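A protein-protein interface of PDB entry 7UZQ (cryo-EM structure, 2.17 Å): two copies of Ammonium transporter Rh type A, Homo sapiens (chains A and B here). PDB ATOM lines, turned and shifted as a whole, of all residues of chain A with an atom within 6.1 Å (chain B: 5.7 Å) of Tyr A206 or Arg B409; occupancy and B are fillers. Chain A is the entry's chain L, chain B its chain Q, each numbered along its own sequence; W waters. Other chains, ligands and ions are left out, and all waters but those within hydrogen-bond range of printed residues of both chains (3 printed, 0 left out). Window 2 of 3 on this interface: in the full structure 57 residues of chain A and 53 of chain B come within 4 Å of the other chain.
Water W3 lies within hydrogen-bond range of the side-chain hydroxyl (OG) of Ser A207 (2.6 Å) and the side-chain hydroxyl (OH) of Tyr B205 (2.6 Å).
Water W1 lies within hydrogen-bond range of the backbone NH of Tyr A206, the side-chain hydroxyl of Tyr B206 and the backbone NH of Tyr A205.
Water W2 bridges the guanidinium group of Arg A409 (3.2 Å) and the side-chain hydroxyl of Tyr B206 (3.5 Å).
Of the printed residues of chain B, Ala A204 touches Tyr B206.
Tyr A205 touches none of the printed residues of chain B.
Of the printed residues of chain B, Phe A210 touches Tyr B206.
Printed residues of chain A within 4 Å of Ala B204: Thr A408 and Arg A409.
Of the printed residues of chain A, Tyr B205 touches Thr A408 (3.1 Å) and Arg A409 (3.3 Å).
Arg B409 touches just these residues of chain A: Tyr A206 and Arg A409.
The nearest residue of chain A that does not touch Arg B409 is Thr A408 (5.8 Å).
Ala A204 touches Tyr B206, but with the chains exchanged Tyr A206 does not touch Ala B204 (9.9 Å).
Thr A408 touches Ala B204, but with the chains exchanged Ala A204 does not touch Thr B408 (13.0 Å).
Arg A409 touches Ala B204, but with the chains exchanged Ala A204 does not touch Arg B409 (11.0 Å).
Arg A409 touches Tyr B205, but with the chains exchanged Tyr A205 does not touch Arg B409 (7.4 Å).
6 positions are printed for both chains.
Of the 11 pairs that touch across the chains among the printed residues, 4 have their exchanged pair printed and touching as well.
CB of Ala A204 touches OH of Tyr B206, at 3.6 Å.
Tyr A206 touches Tyr B206 (CB to CZ, 3.6 Å).
Phe A210 touches Tyr B206 (CE2 to CD1, 3.7 Å).
O of Thr A408 touches CA of Ala B204, 3.6 Å away.
Ala B204 touches Arg A409.
N of Tyr B205 lies within hydrogen-bond range of O of Thr A408 (3.1 Å).
The chain-end carboxylate (OXT) of Arg A409 lies within salt-bridge range of the guanidinium group (NE) of Arg B409 (2.8 Å).
The chain-end carboxylate (O) of Arg A409 lies within hydrogen-bond range of the backbone NH (N) of Tyr B205 (3.3 Å).
OH of Tyr B206 lies within hydrogen-bond range of OG of Ser A207.
The side-chain hydroxyl of Tyr A206 lies within hydrogen-bond range of the chain-end carboxylate of Arg B409 (2.5 Å).
NH2 of Arg A409 sits at hydrogen-bond distance from OH of Tyr B206, at 2.7 Å.
Printed residues of chain A that touch a printed residue of chain B: Ala A204, Tyr A206, Ser A207, Phe A210, Thr A408 and Arg A409.
Hydrophobic or aromatic side chains of chain A within 4 Å of the printed part of chain B: Ala A204, Tyr A206 and Phe A210.
Of the 10 printed residues of chain B, 4 touch a printed residue of chain A.
Printed residues of chain B that touch a printed residue of chain A: Ala B204, Tyr B205, Tyr B206 and Arg B409.
Along chain B the printed residues that touch a printed residue of chain A span positions 204 to 409.
OG of Ser B207 is in hydrogen-bond range of NH2 of Arg B409.
The guanidinium group (NH1) of Arg B409 lies within hydrogen-bond range of the backbone carbonyl oxygen (O) of Lys B73 (3.2 Å).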
ATOM      1  N   ALA A 204      -8.111  18.781 -34.001  1.00  0.00           N
ATOM      2  CA  ALA A 204      -8.300  19.892 -33.089  1.00  0.00           C
ATOM      3  C   ALA A 204      -8.098  21.178 -33.873  1.00  0.00           C
ATOM      4  O   ALA A 204      -7.576  21.169 -34.988  1.00  0.00           O
ATOM      5  CB  ALA A 204      -7.340  19.816 -31.895  1.00  0.00           C
ATOM      6  N   TYR A 205      -8.535  22.288 -33.284  1.00  0.00           N
ATOM      7  CA  TYR A 205      -8.522  23.562 -33.991  1.00  0.00           C
ATOM      8  C   TYR A 205      -7.105  23.954 -34.412  1.00  0.00           C
ATOM      9  O   TYR A 205      -6.795  24.077 -35.607  1.00  0.00           O
ATOM     10  CB  TYR A 205      -9.155  24.633 -33.102  1.00  0.00           C
ATOM     11  CG  TYR A 205      -9.364  25.940 -33.801  1.00  0.00           C
ATOM     12  CD1 TYR A 205     -10.215  26.034 -34.894  1.00  0.00           C
ATOM     13  CD2 TYR A 205      -8.709  27.082 -33.377  1.00  0.00           C
ATOM     14  CE1 TYR A 205     -10.398  27.226 -35.545  1.00  0.00           C
ATOM     15  CE2 TYR A 205      -8.889  28.282 -34.024  1.00  0.00           C
ATOM     16  CZ  TYR A 205      -9.737  28.348 -35.105  1.00  0.00           C
ATOM     17  OH  TYR A 205      -9.926  29.539 -35.754  1.00  0.00           O
ATOM     18  N   TYR A 206      -6.222  24.140 -33.430  1.00  0.00           N
ATOM     19  CA  TYR A 206      -4.848  24.508 -33.742  1.00  0.00           C
ATOM     20  C   TYR A 206      -4.118  23.401 -34.495  1.00  0.00           C
ATOM     21  O   TYR A 206      -3.194  23.685 -35.262  1.00  0.00           O
ATOM     22  CB  TYR A 206      -4.102  24.871 -32.459  1.00  0.00           C
ATOM     23  CG  TYR A 206      -4.661  26.063 -31.704  1.00  0.00           C
ATOM     24  CD1 TYR A 206      -5.174  27.168 -32.377  1.00  0.00           C
ATOM     25  CD2 TYR A 206      -4.663  26.086 -30.316  1.00  0.00           C
ATOM     26  CE1 TYR A 206      -5.673  28.250 -31.693  1.00  0.00           C
ATOM     27  CE2 TYR A 206      -5.160  27.167 -29.624  1.00  0.00           C
ATOM     28  CZ  TYR A 206      -5.663  28.246 -30.316  1.00  0.00           C
ATOM     29  OH  TYR A 206      -6.161  29.326 -29.632  1.00  0.00           O
ATOM     30  N   SER A 207      -4.513  22.141 -34.302  1.00  0.00           N
ATOM     31  CA  SER A 207      -3.901  21.056 -35.064  1.00  0.00           C
ATOM     32  C   SER A 207      -4.207  21.183 -36.552  1.00  0.00           C
ATOM     33  O   SER A 207      -3.327  20.981 -37.395  1.00  0.00           O
ATOM     34  CB  SER A 207      -4.370  19.701 -34.534  1.00  0.00           C
ATOM     35  OG  SER A 207      -3.806  19.422 -33.268  1.00  0.00           O
ATOM     36  N   ASP A 208      -5.453  21.518 -36.898  1.00  0.00           N
ATOM     37  CA  ASP A 208      -5.774  21.778 -38.298  1.00  0.00           C
ATOM     38  C   ASP A 208      -4.994  22.978 -38.813  1.00  0.00           C
ATOM     39  O   ASP A 208      -4.534  22.990 -39.966  1.00  0.00           O
ATOM     40  CB  ASP A 208      -7.276  22.000 -38.465  1.00  0.00           C
ATOM     41  CG  ASP A 208      -8.063  20.712 -38.429  1.00  0.00           C
ATOM     42  OD1 ASP A 208      -7.557  19.684 -38.920  1.00  0.00           O
ATOM     43  OD2 ASP A 208      -9.192  20.719 -37.903  1.00  0.00           O
ATOM     44  N   LEU A 209      -4.818  23.992 -37.966  1.00  0.00           N
ATOM     45  CA  LEU A 209      -3.998  25.128 -38.371  1.00  0.00           C
ATOM     46  C   LEU A 209      -2.577  24.686 -38.717  1.00  0.00           C
ATOM     47  O   LEU A 209      -2.010  25.113 -39.729  1.00  0.00           O
ATOM     48  CB  LEU A 209      -3.984  26.182 -37.268  1.00  0.00           C
ATOM     49  CG  LEU A 209      -3.229  27.477 -37.563  1.00  0.00           C
ATOM     50  CD1 LEU A 209      -3.704  28.123 -38.855  1.00  0.00           C
ATOM     51  CD2 LEU A 209      -3.388  28.431 -36.400  1.00  0.00           C
ATOM     52  N   PHE A 210      -1.984  23.830 -37.885  1.00  0.00           N
ATOM     53  CA  PHE A 210      -0.641  23.334 -38.172  1.00  0.00           C
ATOM     54  C   PHE A 210      -0.618  22.509 -39.454  1.00  0.00           C
ATOM     55  O   PHE A 210       0.330  22.595 -40.239  1.00  0.00           O
ATOM     56  CB  PHE A 210      -0.116  22.506 -36.999  1.00  0.00           C
ATOM     57  CG  PHE A 210       0.683  23.301 -36.014  1.00  0.00           C
ATOM     58  CD1 PHE A 210       2.034  23.511 -36.208  1.00  0.00           C
ATOM     59  CD2 PHE A 210       0.078  23.852 -34.897  1.00  0.00           C
ATOM     60  CE1 PHE A 210       2.770  24.249 -35.305  1.00  0.00           C
ATOM     61  CE2 PHE A 210       0.808  24.589 -33.990  1.00  0.00           C
ATOM     62  CZ  PHE A 210       2.156  24.785 -34.191  1.00  0.00           C
ATOM     63  N   ALA A 211      -1.651  21.697 -39.675  1.00  0.00           N
ATOM     64  CA  ALA A 211      -1.711  20.887 -40.886  1.00  0.00           C
ATOM     65  C   ALA A 211      -1.740  21.752 -42.139  1.00  0.00           C
ATOM     66  O   ALA A 211      -1.205  21.359 -43.187  1.00  0.00           O
ATOM     67  CB  ALA A 211      -2.927  19.967 -40.836  1.00  0.00           C
ATOM     68  N   THR A 408       0.344  20.373 -20.733  1.00  0.00           N
ATOM     69  CA  THR A 408      -0.680  21.267 -21.249  1.00  0.00           C
ATOM     70  C   THR A 408      -0.501  21.411 -22.755  1.00  0.00           C
ATOM     71  O   THR A 408       0.538  21.061 -23.319  1.00  0.00           O
ATOM     72  CB  THR A 408      -0.629  22.648 -20.575  1.00  0.00           C
ATOM     73  OG1 THR A 408       0.583  23.319 -20.939  1.00  0.00           O
ATOM     74  CG2 THR A 408      -0.717  22.520 -19.056  1.00  0.00           C
ATOM     75  N   ARG A 409      -1.532  21.939 -23.402  1.00  0.00           N
ATOM     76  CA  ARG A 409      -1.546  22.076 -24.851  1.00  0.00           C
ATOM     77  C   ARG A 409      -0.904  23.390 -25.295  1.00  0.00           C
ATOM     78  O   ARG A 409      -0.099  23.435 -26.224  1.00  0.00           O
ATOM     79  CB  ARG A 409      -2.978  21.990 -25.381  1.00  0.00           C
ATOM     80  CG  ARG A 409      -3.782  20.785 -24.894  1.00  0.00           C
ATOM     81  CD  ARG A 409      -3.514  19.559 -25.732  1.00  0.00           C
ATOM     82  NE  ARG A 409      -4.017  19.710 -27.092  1.00  0.00           N
ATOM     83  CZ  ARG A 409      -3.879  18.805 -28.051  1.00  0.00           C
ATOM     84  NH1 ARG A 409      -3.284  17.644 -27.828  1.00  0.00           N
ATOM     85  NH2 ARG A 409      -4.352  19.072 -29.263  1.00  0.00           N
ATOM     86  OXT ARG A 409      -1.172  24.446 -24.731  1.00  0.00           O
ATOM     87  N   LYS B  73       6.747  27.246 -22.967  1.00  0.00           N
ATOM     88  CA  LYS B  73       5.299  27.379 -23.074  1.00  0.00           C
ATOM     89  C   LYS B  73       4.856  28.836 -22.984  1.00  0.00           C
ATOM     90  O   LYS B  73       3.886  29.231 -23.636  1.00  0.00           O
ATOM     91  CB  LYS B  73       4.617  26.536 -21.998  1.00  0.00           C
ATOM     92  CG  LYS B  73       4.707  27.114 -20.606  1.00  0.00           C
ATOM     93  CD  LYS B  73       4.359  26.095 -19.556  1.00  0.00           C
ATOM     94  CE  LYS B  73       3.441  26.628 -18.485  1.00  0.00           C
ATOM     95  NZ  LYS B  73       4.089  27.743 -17.752  1.00  0.00           N
ATOM     96  N   LYS B  74       5.554  29.651 -22.192  1.00  0.00           N
ATOM     97  CA  LYS B  74       5.175  31.039 -21.964  1.00  0.00           C
ATOM     98  C   LYS B  74       6.181  32.035 -22.536  1.00  0.00           C
ATOM     99  O   LYS B  74       6.160  33.208 -22.155  1.00  0.00           O
ATOM    100  CB  LYS B  74       4.983  31.281 -20.465  1.00  0.00           C
ATOM    101  CG  LYS B  74       3.623  30.856 -19.957  1.00  0.00           C
ATOM    102  CD  LYS B  74       3.560  30.854 -18.446  1.00  0.00           C
ATOM    103  CE  LYS B  74       3.371  32.258 -17.902  1.00  0.00           C
ATOM    104  NZ  LYS B  74       3.536  32.317 -16.427  1.00  0.00           N
ATOM    105  N   ALA B 204       5.080  22.981 -23.997  1.00  0.00           N
ATOM    106  CA  ALA B 204       3.679  22.667 -24.219  1.00  0.00           C
ATOM    107  C   ALA B 204       3.548  22.034 -25.598  1.00  0.00           C
ATOM    108  O   ALA B 204       4.433  22.164 -26.446  1.00  0.00           O
ATOM    109  CB  ALA B 204       2.790  23.913 -24.096  1.00  0.00           C
ATOM    110  N   TYR B 205       2.434  21.332 -25.801  1.00  0.00           N
ATOM    111  CA  TYR B 205       2.220  20.550 -27.017  1.00  0.00           C
ATOM    112  C   TYR B 205       2.445  21.382 -28.282  1.00  0.00           C
ATOM    113  O   TYR B 205       3.317  21.079 -29.111  1.00  0.00           O
ATOM    114  CB  TYR B 205       0.801  19.981 -26.981  1.00  0.00           C
ATOM    115  CG  TYR B 205       0.444  19.110 -28.152  1.00  0.00           C
ATOM    116  CD1 TYR B 205       0.873  17.796 -28.219  1.00  0.00           C
ATOM    117  CD2 TYR B 205      -0.323  19.607 -29.195  1.00  0.00           C
ATOM    118  CE1 TYR B 205       0.543  16.998 -29.289  1.00  0.00           C
ATOM    119  CE2 TYR B 205      -0.654  18.821 -30.267  1.00  0.00           C
ATOM    120  CZ  TYR B 205      -0.218  17.515 -30.311  1.00  0.00           C
ATOM    121  OH  TYR B 205      -0.549  16.725 -31.379  1.00  0.00           O
ATOM    122  N   TYR B 206       1.668  22.452 -28.438  1.00  0.00           N
ATOM    123  CA  TYR B 206       1.775  23.260 -29.647  1.00  0.00           C
ATOM    124  C   TYR B 206       3.074  24.058 -29.678  1.00  0.00           C
ATOM    125  O   TYR B 206       3.602  24.338 -30.764  1.00  0.00           O
ATOM    126  CB  TYR B 206       0.548  24.163 -29.770  1.00  0.00           C
ATOM    127  CG  TYR B 206      -0.715  23.387 -30.070  1.00  0.00           C
ATOM    128  CD1 TYR B 206      -0.839  22.668 -31.255  1.00  0.00           C
ATOM    129  CD2 TYR B 206      -1.778  23.358 -29.174  1.00  0.00           C
ATOM    130  CE1 TYR B 206      -1.971  21.954 -31.538  1.00  0.00           C
ATOM    131  CE2 TYR B 206      -2.922  22.645 -29.453  1.00  0.00           C
ATOM    132  CZ  TYR B 206      -3.011  21.939 -30.638  1.00  0.00           C
ATOM    133  OH  TYR B 206      -4.141  21.223 -30.944  1.00  0.00           O
ATOM    134  N   SER B 207       3.618  24.406 -28.512  1.00  0.00           N
ATOM    135  CA  SER B 207       4.945  25.012 -28.476  1.00  0.00           C
ATOM    136  C   SER B 207       5.987  24.066 -29.062  1.00  0.00           C
ATOM    137  O   SER B 207       6.877  24.492 -29.805  1.00  0.00           O
ATOM    138  CB  SER B 207       5.316  25.392 -27.044  1.00  0.00           C
ATOM    139  OG  SER B 207       4.309  26.181 -26.445  1.00  0.00           O
ATOM    140  N   PRO B 406      -1.779  37.670 -25.204  1.00  0.00           N
ATOM    141  CA  PRO B 406      -3.233  37.470 -25.243  1.00  0.00           C
ATOM    142  C   PRO B 406      -3.720  36.646 -24.062  1.00  0.00           C
ATOM    143  O   PRO B 406      -3.025  35.760 -23.563  1.00  0.00           O
ATOM    144  CB  PRO B 406      -3.459  36.729 -26.567  1.00  0.00           C
ATOM    145  CG  PRO B 406      -2.270  37.028 -27.383  1.00  0.00           C
ATOM    146  CD  PRO B 406      -1.137  37.160 -26.428  1.00  0.00           C
ATOM    147  N   LYS B 407      -4.937  36.956 -23.614  1.00  0.00           N
ATOM    148  CA  LYS B 407      -5.567  36.167 -22.563  1.00  0.00           C
ATOM    149  C   LYS B 407      -5.743  34.722 -23.006  1.00  0.00           C
ATOM    150  O   LYS B 407      -5.614  33.801 -22.193  1.00  0.00           O
ATOM    151  CB  LYS B 407      -6.913  36.806 -22.189  1.00  0.00           C
ATOM    152  CG  LYS B 407      -7.935  35.949 -21.409  1.00  0.00           C
ATOM    153  CD  LYS B 407      -9.359  36.130 -21.945  1.00  0.00           C
ATOM    154  CE  LYS B 407     -10.020  37.405 -21.434  1.00  0.00           C
ATOM    155  NZ  LYS B 407     -11.488  37.233 -21.262  1.00  0.00           N
ATOM    156  N   THR B 408      -6.023  34.507 -24.286  1.00  0.00           N
ATOM    157  CA  THR B 408      -6.313  33.185 -24.818  1.00  0.00           C
ATOM    158  C   THR B 408      -5.051  32.537 -25.370  1.00  0.00           C
ATOM    159  O   THR B 408      -4.261  33.178 -26.066  1.00  0.00           O
ATOM    160  CB  THR B 408      -7.370  33.282 -25.921  1.00  0.00           C
ATOM    161  OG1 THR B 408      -8.558  33.892 -25.399  1.00  0.00           O
ATOM    162  CG2 THR B 408      -7.705  31.908 -26.483  1.00  0.00           C
ATOM    163  N   ARG B 409      -4.870  31.260 -25.061  1.00  0.00           N
ATOM    164  CA  ARG B 409      -3.795  30.482 -25.664  1.00  0.00           C
ATOM    165  C   ARG B 409      -4.204  30.074 -27.085  1.00  0.00           C
ATOM    166  O   ARG B 409      -3.416  30.149 -28.022  1.00  0.00           O
ATOM    167  CB  ARG B 409      -3.471  29.253 -24.811  1.00  0.00           C
ATOM    168  CG  ARG B 409      -2.503  28.255 -25.451  1.00  0.00           C
ATOM    169  CD  ARG B 409      -1.275  28.029 -24.609  1.00  0.00           C
ATOM    170  NE  ARG B 409      -0.384  27.065 -25.251  1.00  0.00           N
ATOM    171  CZ  ARG B 409       0.852  27.305 -25.673  1.00  0.00           C
ATOM    172  NH1 ARG B 409       1.433  28.486 -25.514  1.00  0.00           N
ATOM    173  NH2 ARG B 409       1.525  26.336 -26.283  1.00  0.00           N
ATOM    174  OXT ARG B 409      -5.335  29.658 -27.330  1.00  0.00           O
HETATM  175  O   HOH W   1      -6.572  23.301 -30.860  1.00  0.00           O
HETATM  176  O   HOH W   2      -6.263  21.688 -28.206  1.00  0.00           O
HETATM  177  O   HOH W   3      -1.810  17.783 -33.453  1.00  0.00           O
